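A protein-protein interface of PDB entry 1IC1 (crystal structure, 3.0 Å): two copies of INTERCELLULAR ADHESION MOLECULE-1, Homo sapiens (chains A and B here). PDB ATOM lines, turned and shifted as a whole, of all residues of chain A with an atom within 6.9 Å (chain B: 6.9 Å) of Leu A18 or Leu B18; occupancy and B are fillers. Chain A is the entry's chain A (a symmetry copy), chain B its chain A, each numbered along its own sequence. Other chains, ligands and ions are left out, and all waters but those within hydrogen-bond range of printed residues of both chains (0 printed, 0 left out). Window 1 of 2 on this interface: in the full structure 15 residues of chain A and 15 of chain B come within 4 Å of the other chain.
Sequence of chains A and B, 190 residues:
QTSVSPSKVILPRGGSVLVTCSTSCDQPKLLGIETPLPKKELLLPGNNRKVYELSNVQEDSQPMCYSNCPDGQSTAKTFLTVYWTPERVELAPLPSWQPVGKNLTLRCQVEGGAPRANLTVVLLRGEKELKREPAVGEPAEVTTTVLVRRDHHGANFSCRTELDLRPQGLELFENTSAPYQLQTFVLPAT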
ATOM      1  N   SER A   5       7.304  -2.559  19.349  1.00  0.00           N
ATOM      2  CA  SER A   5       7.115  -2.397  17.933  1.00  0.00           C
ATOM      3  C   SER A   5       6.031  -3.351  17.459  1.00  0.00           C
ATOM      4  O   SER A   5       5.999  -4.531  17.861  1.00  0.00           O
ATOM      5  CB  SER A   5       8.426  -2.650  17.205  1.00  0.00           C
ATOM      6  OG  SER A   5       8.328  -3.774  16.360  1.00  0.00           O
ATOM      7  N   PRO A   6       5.059  -2.826  16.695  1.00  0.00           N
ATOM      8  CA  PRO A   6       4.957  -1.420  16.306  1.00  0.00           C
ATOM      9  C   PRO A   6       4.452  -0.582  17.448  1.00  0.00           C
ATOM     10  O   PRO A   6       4.023  -1.084  18.475  1.00  0.00           O
ATOM     11  CB  PRO A   6       3.931  -1.462  15.196  1.00  0.00           C
ATOM     12  CG  PRO A   6       3.038  -2.509  15.672  1.00  0.00           C
ATOM     13  CD  PRO A   6       3.990  -3.597  16.058  1.00  0.00           C
ATOM     14  N   VAL A   9      -0.833   0.897  15.559  1.00  0.00           N
ATOM     15  CA  VAL A   9      -1.450  -0.186  14.755  1.00  0.00           C
ATOM     16  C   VAL A   9      -2.930   0.088  14.415  1.00  0.00           C
ATOM     17  O   VAL A   9      -3.761   0.422  15.289  1.00  0.00           O
ATOM     18  CB  VAL A   9      -1.463  -1.582  15.468  1.00  0.00           C
ATOM     19  CG1 VAL A   9      -1.868  -2.695  14.460  1.00  0.00           C
ATOM     20  CG2 VAL A   9      -0.139  -1.862  16.138  1.00  0.00           C
ATOM     21  N   SER A  16      -6.186  -9.449  15.343  1.00  0.00           N
ATOM     22  CA  SER A  16      -5.180  -9.711  16.338  1.00  0.00           C
ATOM     23  C   SER A  16      -3.907  -9.058  15.823  1.00  0.00           C
ATOM     24  O   SER A  16      -3.861  -8.649  14.672  1.00  0.00           O
ATOM     25  CB  SER A  16      -4.936 -11.197  16.337  1.00  0.00           C
ATOM     26  OG  SER A  16      -4.251 -11.488  15.115  1.00  0.00           O
ATOM     27  N   VAL A  17      -2.851  -9.046  16.638  1.00  0.00           N
ATOM     28  CA  VAL A  17      -1.559  -8.514  16.218  1.00  0.00           C
ATOM     29  C   VAL A  17      -0.457  -9.107  17.027  1.00  0.00           C
ATOM     30  O   VAL A  17      -0.674  -9.525  18.179  1.00  0.00           O
ATOM     31  CB  VAL A  17      -1.362  -7.013  16.488  1.00  0.00           C
ATOM     32  CG1 VAL A  17      -1.016  -6.297  15.221  1.00  0.00           C
ATOM     33  CG2 VAL A  17      -2.505  -6.420  17.221  1.00  0.00           C
ATOM     34  N   LEU A  18       0.743  -8.984  16.460  1.00  0.00           N
ATOM     35  CA  LEU A  18       1.987  -9.399  17.098  1.00  0.00           C
ATOM     36  C   LEU A  18       2.671  -8.146  17.661  1.00  0.00           C
ATOM     37  O   LEU A  18       2.803  -7.121  16.965  1.00  0.00           O
ATOM     38  CB  LEU A  18       2.928 -10.004  16.086  1.00  0.00           C
ATOM     39  CG  LEU A  18       2.413 -11.329  15.640  1.00  0.00           C
ATOM     40  CD1 LEU A  18       3.512 -12.028  14.793  1.00  0.00           C
ATOM     41  CD2 LEU A  18       1.979 -12.090  16.961  1.00  0.00           C
ATOM     42  N   VAL A  19       3.077  -8.192  18.923  1.00  0.00           N
ATOM     43  CA  VAL A  19       3.767  -7.051  19.512  1.00  0.00           C
ATOM     44  C   VAL A  19       5.066  -7.567  20.105  1.00  0.00           C
ATOM     45  O   VAL A  19       5.110  -8.662  20.649  1.00  0.00           O
ATOM     46  CB  VAL A  19       2.939  -6.409  20.608  1.00  0.00           C
ATOM     47  CG1 VAL A  19       3.677  -5.241  21.148  1.00  0.00           C
ATOM     48  CG2 VAL A  19       1.598  -5.994  20.048  1.00  0.00           C
ATOM     49  N   THR A  20       6.145  -6.836  19.899  1.00  0.00           N
ATOM     50  CA  THR A  20       7.408  -7.262  20.450  1.00  0.00           C
ATOM     51  C   THR A  20       7.765  -6.259  21.499  1.00  0.00           C
ATOM     52  O   THR A  20       7.547  -5.056  21.305  1.00  0.00           O
ATOM     53  CB  THR A  20       8.456  -7.247  19.408  1.00  0.00           C
ATOM     54  OG1 THR A  20       8.043  -8.102  18.328  1.00  0.00           O
ATOM     55  CG2 THR A  20       9.758  -7.728  20.005  1.00  0.00           C
ATOM     56  N   LYS A  40      -0.547 -14.253  23.919  1.00  0.00           N
ATOM     57  CA  LYS A  40       0.108 -15.541  23.722  1.00  0.00           C
ATOM     58  C   LYS A  40       1.550 -15.229  23.492  1.00  0.00           C
ATOM     59  O   LYS A  40       1.856 -14.369  22.668  1.00  0.00           O
ATOM     60  CB  LYS A  40      -0.422 -16.148  22.440  1.00  0.00           C
ATOM     61  CG  LYS A  40      -0.059 -17.587  22.181  1.00  0.00           C
ATOM     62  CD  LYS A  40      -0.623 -18.011  20.815  1.00  0.00           C
ATOM     63  CE  LYS A  40      -2.086 -17.555  20.619  1.00  0.00           C
ATOM     64  NZ  LYS A  40      -2.627 -17.725  19.212  1.00  0.00           N
ATOM     65  N   LEU A  42       5.621 -16.237  22.272  1.00  0.00           N
ATOM     66  CA  LEU A  42       6.358 -17.137  21.334  1.00  0.00           C
ATOM     67  C   LEU A  42       7.921 -17.400  21.563  1.00  0.00           C
ATOM     68  O   LEU A  42       8.577 -16.514  22.182  1.00  0.00           O
ATOM     69  CB  LEU A  42       6.097 -16.594  19.916  1.00  0.00           C
ATOM     70  CG  LEU A  42       4.670 -16.052  19.717  1.00  0.00           C
ATOM     71  CD1 LEU A  42       4.540 -15.239  18.474  1.00  0.00           C
ATOM     72  CD2 LEU A  42       3.704 -17.177  19.669  1.00  0.00           C
ATOM     73  N   LEU A  44      10.990 -16.670  20.881  1.00  0.00           N
ATOM     74  CA  LEU A  44      11.920 -15.776  20.211  1.00  0.00           C
ATOM     75  C   LEU A  44      13.254 -15.746  20.943  1.00  0.00           C
ATOM     76  O   LEU A  44      13.303 -15.533  22.164  1.00  0.00           O
ATOM     77  CB  LEU A  44      11.359 -14.294  20.244  1.00  0.00           C
ATOM     78  CG  LEU A  44      12.284 -13.261  19.597  1.00  0.00           C
ATOM     79  CD1 LEU A  44      12.440 -13.458  18.089  1.00  0.00           C
ATOM     80  CD2 LEU A  44      11.782 -11.823  19.775  1.00  0.00           C
ATOM     81  N   ARG A  49      14.046  -9.931  24.346  1.00  0.00           N
ATOM     82  CA  ARG A  49      12.910  -9.830  23.408  1.00  0.00           C
ATOM     83  C   ARG A  49      11.798 -10.867  23.623  1.00  0.00           C
ATOM     84  O   ARG A  49      12.062 -12.068  23.631  1.00  0.00           O
ATOM     85  CB  ARG A  49      13.411 -10.001  21.974  1.00  0.00           C
ATOM     86  CG  ARG A  49      13.978  -8.741  21.355  1.00  0.00           C
ATOM     87  CD  ARG A  49      14.732  -9.049  20.091  1.00  0.00           C
ATOM     88  NE  ARG A  49      14.729  -7.905  19.214  1.00  0.00           N
ATOM     89  CZ  ARG A  49      14.280  -7.962  17.969  1.00  0.00           C
ATOM     90  NH1 ARG A  49      13.826  -9.125  17.489  1.00  0.00           N
ATOM     91  NH2 ARG A  49      14.216  -6.851  17.222  1.00  0.00           N
ATOM     92  N   VAL A  51       7.648 -11.772  22.261  1.00  0.00           N
ATOM     93  CA  VAL A  51       6.621 -11.516  21.250  1.00  0.00           C
ATOM     94  C   VAL A  51       5.266 -12.093  21.664  1.00  0.00           C
ATOM     95  O   VAL A  51       5.112 -13.298  21.853  1.00  0.00           O
ATOM     96  CB  VAL A  51       7.003 -12.106  19.881  1.00  0.00           C
ATOM     97  CG1 VAL A  51       5.999 -11.676  18.846  1.00  0.00           C
ATOM     98  CG2 VAL A  51       8.364 -11.661  19.478  1.00  0.00           C
ATOM     99  N   TYR A  52       4.274 -11.226  21.761  1.00  0.00           N
ATOM    100  CA  TYR A  52       2.919 -11.587  22.184  1.00  0.00           C
ATOM    101  C   TYR A  52       1.932 -11.462  21.019  1.00  0.00           C
ATOM    102  O   TYR A  52       2.160 -10.676  20.099  1.00  0.00           O
ATOM    103  CB  TYR A  52       2.511 -10.636  23.322  1.00  0.00           C
ATOM    104  CG  TYR A  52       3.399 -10.773  24.550  1.00  0.00           C
ATOM    105  CD1 TYR A  52       3.181 -11.808  25.445  1.00  0.00           C
ATOM    106  CD2 TYR A  52       4.498  -9.930  24.767  1.00  0.00           C
ATOM    107  CE1 TYR A  52       4.010 -12.024  26.506  1.00  0.00           C
ATOM    108  CE2 TYR A  52       5.343 -10.138  25.839  1.00  0.00           C
ATOM    109  CZ  TYR A  52       5.088 -11.205  26.711  1.00  0.00           C
ATOM    110  OH  TYR A  52       5.907 -11.514  27.789  1.00  0.00           O
ATOM    111  N   GLU A  53       0.862 -12.247  21.037  1.00  0.00           N
ATOM    112  CA  GLU A  53      -0.128 -12.208  19.976  1.00  0.00           C
ATOM    113  C   GLU A  53      -1.353 -11.750  20.662  1.00  0.00           C
ATOM    114  O   GLU A  53      -1.979 -12.512  21.393  1.00  0.00           O
ATOM    115  CB  GLU A  53      -0.422 -13.590  19.412  1.00  0.00           C
ATOM    116  CG  GLU A  53      -1.407 -13.552  18.238  1.00  0.00           C
ATOM    117  CD  GLU A  53      -1.781 -14.929  17.651  1.00  0.00           C
ATOM    118  OE1 GLU A  53      -1.008 -15.572  16.881  1.00  0.00           O
ATOM    119  OE2 GLU A  53      -2.912 -15.369  17.945  1.00  0.00           O
ATOM    120  N   LEU A  54      -1.694 -10.496  20.472  1.00  0.00           N
ATOM    121  CA  LEU A  54      -2.872  -9.989  21.128  1.00  0.00           C
ATOM    122  C   LEU A  54      -4.041 -10.464  20.277  1.00  0.00           C
ATOM    123  O   LEU A  54      -3.901 -10.542  19.045  1.00  0.00           O
ATOM    124  CB  LEU A  54      -2.737  -8.479  21.302  1.00  0.00           C
ATOM    125  CG  LEU A  54      -1.458  -8.220  22.123  1.00  0.00           C
ATOM    126  CD1 LEU A  54      -1.479  -6.803  22.584  1.00  0.00           C
ATOM    127  CD2 LEU A  54      -1.327  -9.190  23.331  1.00  0.00           C
ATOM    128  N   SER B   5       0.197 -12.846   6.707  1.00  0.00           N
ATOM    129  CA  SER B   5      -0.172 -11.576   7.271  1.00  0.00           C
ATOM    130  C   SER B   5       1.042 -10.954   7.943  1.00  0.00           C
ATOM    131  O   SER B   5       1.802 -11.642   8.652  1.00  0.00           O
ATOM    132  CB  SER B   5      -1.311 -11.761   8.261  1.00  0.00           C
ATOM    133  OG  SER B   5      -0.911 -11.413   9.567  1.00  0.00           O
ATOM    134  N   PRO B   6       1.311  -9.674   7.634  1.00  0.00           N
ATOM    135  CA  PRO B   6       0.546  -8.852   6.698  1.00  0.00           C
ATOM    136  C   PRO B   6       0.866  -9.217   5.275  1.00  0.00           C
ATOM    137  O   PRO B   6       1.784  -9.972   4.995  1.00  0.00           O
ATOM    138  CB  PRO B   6       1.045  -7.458   7.004  1.00  0.00           C
ATOM    139  CG  PRO B   6       2.446  -7.715   7.304  1.00  0.00           C
ATOM    140  CD  PRO B   6       2.368  -8.870   8.252  1.00  0.00           C
ATOM    141  N   VAL B   9       3.739  -4.505   3.482  1.00  0.00           N
ATOM    142  CA  VAL B   9       4.545  -3.906   4.574  1.00  0.00           C
ATOM    143  C   VAL B   9       5.480  -2.780   4.082  1.00  0.00           C
ATOM    144  O   VAL B   9       6.240  -2.931   3.099  1.00  0.00           O
ATOM    145  CB  VAL B   9       5.497  -4.921   5.295  1.00  0.00           C
ATOM    146  CG1 VAL B   9       6.087  -4.281   6.584  1.00  0.00           C
ATOM    147  CG2 VAL B   9       4.791  -6.227   5.568  1.00  0.00           C
ATOM    148  N   SER B  16      13.301  -4.963  10.123  1.00  0.00           N
ATOM    149  CA  SER B  16      12.940  -6.356  10.112  1.00  0.00           C
ATOM    150  C   SER B  16      11.427  -6.393  10.261  1.00  0.00           C
ATOM    151  O   SER B  16      10.825  -5.373  10.562  1.00  0.00           O
ATOM    152  CB  SER B  16      13.514  -6.969  11.362  1.00  0.00           C
ATOM    153  OG  SER B  16      12.740  -6.454  12.451  1.00  0.00           O
ATOM    154  N   VAL B  17      10.829  -7.579  10.145  1.00  0.00           N
ATOM    155  CA  VAL B  17       9.392  -7.741  10.344  1.00  0.00           C
ATOM    156  C   VAL B  17       9.068  -9.146  10.723  1.00  0.00           C
ATOM    157  O   VAL B  17       9.813 -10.080  10.376  1.00  0.00           O
ATOM    158  CB  VAL B  17       8.541  -7.563   9.076  1.00  0.00           C
ATOM    159  CG1 VAL B  17       7.504  -6.506   9.288  1.00  0.00           C
ATOM    160  CG2 VAL B  17       9.373  -7.356   7.867  1.00  0.00           C
ATOM    161  N   LEU B  18       7.872  -9.278  11.296  1.00  0.00           N
ATOM    162  CA  LEU B  18       7.290 -10.562  11.668  1.00  0.00           C
ATOM    163  C   LEU B  18       6.268 -10.950  10.590  1.00  0.00           C
ATOM    164  O   LEU B  18       5.418 -10.131  10.190  1.00  0.00           O
ATOM    165  CB  LEU B  18       6.540 -10.448  12.972  1.00  0.00           C
ATOM    166  CG  LEU B  18       7.499 -10.265  14.098  1.00  0.00           C
ATOM    167  CD1 LEU B  18       6.723 -10.394  15.437  1.00  0.00           C
ATOM    168  CD2 LEU B  18       8.646 -11.334  13.864  1.00  0.00           C
ATOM    169  N   VAL B  19       6.356 -12.172  10.083  1.00  0.00           N
ATOM    170  CA  VAL B  19       5.396 -12.620   9.081  1.00  0.00           C
ATOM    171  C   VAL B  19       4.808 -13.930   9.574  1.00  0.00           C
ATOM    172  O   VAL B  19       5.507 -14.742  10.164  1.00  0.00           O
ATOM    173  CB  VAL B  19       6.062 -12.846   7.739  1.00  0.00           C
ATOM    174  CG1 VAL B  19       5.035 -13.271   6.756  1.00  0.00           C
ATOM    175  CG2 VAL B  19       6.746 -11.573   7.294  1.00  0.00           C
ATOM    176  N   THR B  20       3.506 -14.085   9.438  1.00  0.00           N
ATOM    177  CA  THR B  20       2.887 -15.314   9.871  1.00  0.00           C
ATOM    178  C   THR B  20       2.406 -15.998   8.632  1.00  0.00           C
ATOM    179  O   THR B  20       1.897 -15.337   7.718  1.00  0.00           O
ATOM    180  CB  THR B  20       1.722 -15.028  10.734  1.00  0.00           C
ATOM    181  OG1 THR B  20       2.162 -14.242  11.855  1.00  0.00           O
ATOM    182  CG2 THR B  20       1.115 -16.331  11.198  1.00  0.00           C
ATOM    183  N   LYS B  40      13.924 -16.235  11.107  1.00  0.00           N
ATOM    184  CA  LYS B  40      14.007 -16.841  12.431  1.00  0.00           C
ATOM    185  C   LYS B  40      12.623 -17.303  12.750  1.00  0.00           C
ATOM    186  O   LYS B  40      11.681 -16.528  12.602  1.00  0.00           O
ATOM    187  CB  LYS B  40      14.349 -15.754  13.427  1.00  0.00           C
ATOM    188  CG  LYS B  40      14.726 -16.210  14.813  1.00  0.00           C
ATOM    189  CD  LYS B  40      14.974 -14.978  15.699  1.00  0.00           C
ATOM    190  CE  LYS B  40      15.846 -13.916  14.992  1.00  0.00           C
ATOM    191  NZ  LYS B  40      15.933 -12.580  15.706  1.00  0.00           N
ATOM    192  N   LEU B  42       9.520 -18.778  15.446  1.00  0.00           N
ATOM    193  CA  LEU B  42       9.108 -18.714  16.882  1.00  0.00           C
ATOM    194  C   LEU B  42       8.067 -19.790  17.449  1.00  0.00           C
ATOM    195  O   LEU B  42       7.275 -20.328  16.623  1.00  0.00           O
ATOM    196  CB  LEU B  42       8.599 -17.280  17.124  1.00  0.00           C
ATOM    197  CG  LEU B  42       9.397 -16.206  16.362  1.00  0.00           C
ATOM    198  CD1 LEU B  42       8.697 -14.889  16.338  1.00  0.00           C
ATOM    199  CD2 LEU B  42      10.735 -16.038  16.979  1.00  0.00           C
ATOM    200  N   LEU B  44       5.029 -20.599  18.178  1.00  0.00           N
ATOM    201  CA  LEU B  44       3.617 -20.258  18.113  1.00  0.00           C
ATOM    202  C   LEU B  44       2.762 -21.517  18.112  1.00  0.00           C
ATOM    203  O   LEU B  44       2.988 -22.437  17.312  1.00  0.00           O
ATOM    204  CB  LEU B  44       3.308 -19.507  16.752  1.00  0.00           C
ATOM    205  CG  LEU B  44       1.836 -19.134  16.563  1.00  0.00           C
ATOM    206  CD1 LEU B  44       1.349 -18.088  17.567  1.00  0.00           C
ATOM    207  CD2 LEU B  44       1.547 -18.543  15.179  1.00  0.00           C
ATOM    208  N   ARG B  49       0.167 -22.704  11.957  1.00  0.00           N
ATOM    209  CA  ARG B  49       0.733 -21.342  12.026  1.00  0.00           C
ATOM    210  C   ARG B  49       2.224 -21.277  12.388  1.00  0.00           C
ATOM    211  O   ARG B  49       2.637 -21.815  13.415  1.00  0.00           O
ATOM    212  CB  ARG B  49      -0.019 -20.525  13.074  1.00  0.00           C
ATOM    213  CG  ARG B  49      -1.315 -19.915  12.582  1.00  0.00           C
ATOM    214  CD  ARG B  49      -2.146 -19.407  13.728  1.00  0.00           C
ATOM    215  NE  ARG B  49      -3.006 -18.337  13.288  1.00  0.00           N
ATOM    216  CZ  ARG B  49      -3.001 -17.140  13.855  1.00  0.00           C
ATOM    217  NH1 ARG B  49      -2.184 -16.908  14.888  1.00  0.00           N
ATOM    218  NH2 ARG B  49      -3.754 -16.152  13.353  1.00  0.00           N
ATOM    219  N   VAL B  51       5.587 -18.350  12.549  1.00  0.00           N
ATOM    220  CA  VAL B  51       5.963 -16.936  12.566  1.00  0.00           C
ATOM    221  C   VAL B  51       7.471 -16.752  12.385  1.00  0.00           C
ATOM    222  O   VAL B  51       8.276 -17.217  13.190  1.00  0.00           O
ATOM    223  CB  VAL B  51       5.542 -16.247  13.876  1.00  0.00           C
ATOM    224  CG1 VAL B  51       5.803 -14.768  13.776  1.00  0.00           C
ATOM    225  CG2 VAL B  51       4.101 -16.486  14.156  1.00  0.00           C
ATOM    226  N   TYR B  52       7.845 -16.031  11.344  1.00  0.00           N
ATOM    227  CA  TYR B  52       9.243 -15.781  10.987  1.00  0.00           C
ATOM    228  C   TYR B  52       9.608 -14.309  11.202  1.00  0.00           C
ATOM    229  O   TYR B  52       8.735 -13.442  11.139  1.00  0.00           O
ATOM    230  CB  TYR B  52       9.427 -16.158   9.508  1.00  0.00           C
ATOM    231  CG  TYR B  52       9.167 -17.632   9.237  1.00  0.00           C
ATOM    232  CD1 TYR B  52      10.152 -18.566   9.513  1.00  0.00           C
ATOM    233  CD2 TYR B  52       7.920 -18.095   8.795  1.00  0.00           C
ATOM    234  CE1 TYR B  52       9.929 -19.905   9.377  1.00  0.00           C
ATOM    235  CE2 TYR B  52       7.683 -19.447   8.651  1.00  0.00           C
ATOM    236  CZ  TYR B  52       8.706 -20.356   8.953  1.00  0.00           C
ATOM    237  OH  TYR B  52       8.544 -21.733   8.878  1.00  0.00           O
ATOM    238  N   GLU B  53      10.874 -14.028  11.484  1.00  0.00           N
ATOM    239  CA  GLU B  53      11.318 -12.665  11.711  1.00  0.00           C
ATOM    240  C   GLU B  53      12.270 -12.423  10.609  1.00  0.00           C
ATOM    241  O   GLU B  53      13.389 -12.926  10.631  1.00  0.00           O
ATOM    242  CB  GLU B  53      12.094 -12.521  13.012  1.00  0.00           C
ATOM    243  CG  GLU B  53      12.500 -11.071  13.300  1.00  0.00           C
ATOM    244  CD  GLU B  53      13.330 -10.866  14.585  1.00  0.00           C
ATOM    245  OE1 GLU B  53      12.809 -10.870  15.739  1.00  0.00           O
ATOM    246  OE2 GLU B  53      14.551 -10.658  14.428  1.00  0.00           O
ATOM    247  N   LEU B  54      11.835 -11.684   9.613  1.00  0.00           N
ATOM    248  CA  LEU B  54      12.715 -11.426   8.503  1.00  0.00           C
ATOM    249  C   LEU B  54      13.632 -10.304   8.969  1.00  0.00           C
ATOM    250  O   LEU B  54      13.182  -9.429   9.727  1.00  0.00           O
ATOM    251  CB  LEU B  54      11.879 -11.137   7.258  1.00  0.00           C
ATOM    252  CG  LEU B  54      10.976 -12.362   7.013  1.00  0.00           C
ATOM    253  CD1 LEU B  54      10.402 -12.250   5.642  1.00  0.00           C
ATOM    254  CD2 LEU B  54      11.746 -13.703   7.179  1.00  0.00           C
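The guanidinium group of Arg A49 lies within salt-bridge range of the side-chain carboxylate of Glu B53 (2.7 Å).
The guanidinium group (NH1) of Arg B49 lies within salt-bridge range of the side-chain carboxylate (OE1) of Glu A53.
The backbone carbonyl oxygen of Ser A5 sits at hydrogen-bond distance from the backbone NH of Thr A20.
NZ of Lys B40 is in salt-bridge range of OE2 of Glu B53 (2.7 Å).
The side-chain amino group (NZ) of Lys A40 lies within salt-bridge range of the side-chain carboxylate (OE2) of Glu A53, at 2.7 Å.
O of Ser B5 is in hydrogen-bond range of N of Thr B20 (3.1 Å).
N of Leu B42 sits at hydrogen-bond distance from O of Val B51.
The backbone NH (N) of Leu A42 lies within hydrogen-bond range of the backbone carbonyl oxygen (O) of Val A51 (3.0 Å).
Among the printed residues, merely in contact across the chains: Leu A42 with Leu B44 (3.3 Å), Leu A44 with Leu B42 (3.3 Å), Glu A53 with Leu B44 (3.5 Å), Leu A44 with Glu B53 (3.5 Å), Leu A18 with Leu B18 (3.7 Å), Val A51 with Leu B18 (3.7 Å), Leu A18 with Val B51 (3.7 Å), Leu A44 with Lys B40 (3.8 Å), Lys A40 with Leu B44 (3.8 Å), Leu A42 with Leu B42 (3.8 Å), Thr A20 with Leu B18 (3.9 Å) and Leu A18 with Thr B20 (3.9 Å).
Of chain B, only Leu B18 (3.7 Å), Thr B20 (3.9 Å) and Val B51 (3.7 Å) come within 4 Å of Leu A18.
Leu B18 touches just these residues of chain A: Leu A18, Thr A20 and Val A51.
Printed residues of chain A within 4 Å of Leu B42: Leu A42 and Leu A44.
Of the printed residues of chain B, Glu A53 touches Leu B44 and Arg B49.
Printed residues of chain A within 4 Å of Thr B20: Leu A18 (3.9 Å).
Of the printed residues of chain A, Glu B53 touches Leu A44 and Arg A49.
Printed residues of chain B within 4 Å of Lys A40: Leu B44 (3.8 Å).
Ser B5 touches none of the printed residues of chain A.
The nearest residue of chain B that does not touch Leu A18 is Val B19 (5.5 Å).
Hydrophobic or aromatic side chains of chain B within 4 Å of the printed part of chain A: Leu B18, Leu B42, Leu B44 and Val B51.
Printed residues of chain A that touch a printed residue of chain B: Leu A18, Thr A20, Lys A40, Leu A42, Leu A44, Arg A49, Val A51 and Glu A53.
Hydrophobic or aromatic side chains of chain A that line the printed part of chain B: Leu A18, Leu A42, Leu A44 and Val A51.
Along chain A the printed residues that touch a printed residue of chain B span positions 18 to 53.
Among the printed residues, 14 pairs touch across the chains.
Among the printed residues, Asp or Glu carboxylates within 4 Å of a Lys or Arg side-chain nitrogen of the other chain: Arg A49 with Glu B53 and Glu A53 with Arg B49.
Leu A18 touches Val B51, and with the chains exchanged Val A51 touches Leu B18.
Lys A40 touches Leu B44, and with the chains exchanged Leu A44 touches Lys B40.
Leu B42 touches its own counterpart, Leu A42.
Leu A42 touches Leu B44, and with the chains exchanged Leu A44 touches Leu B42.
Of the 14 pairs that touch across the chains among the printed residues, 14 have their exchanged pair printed and touching as well.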
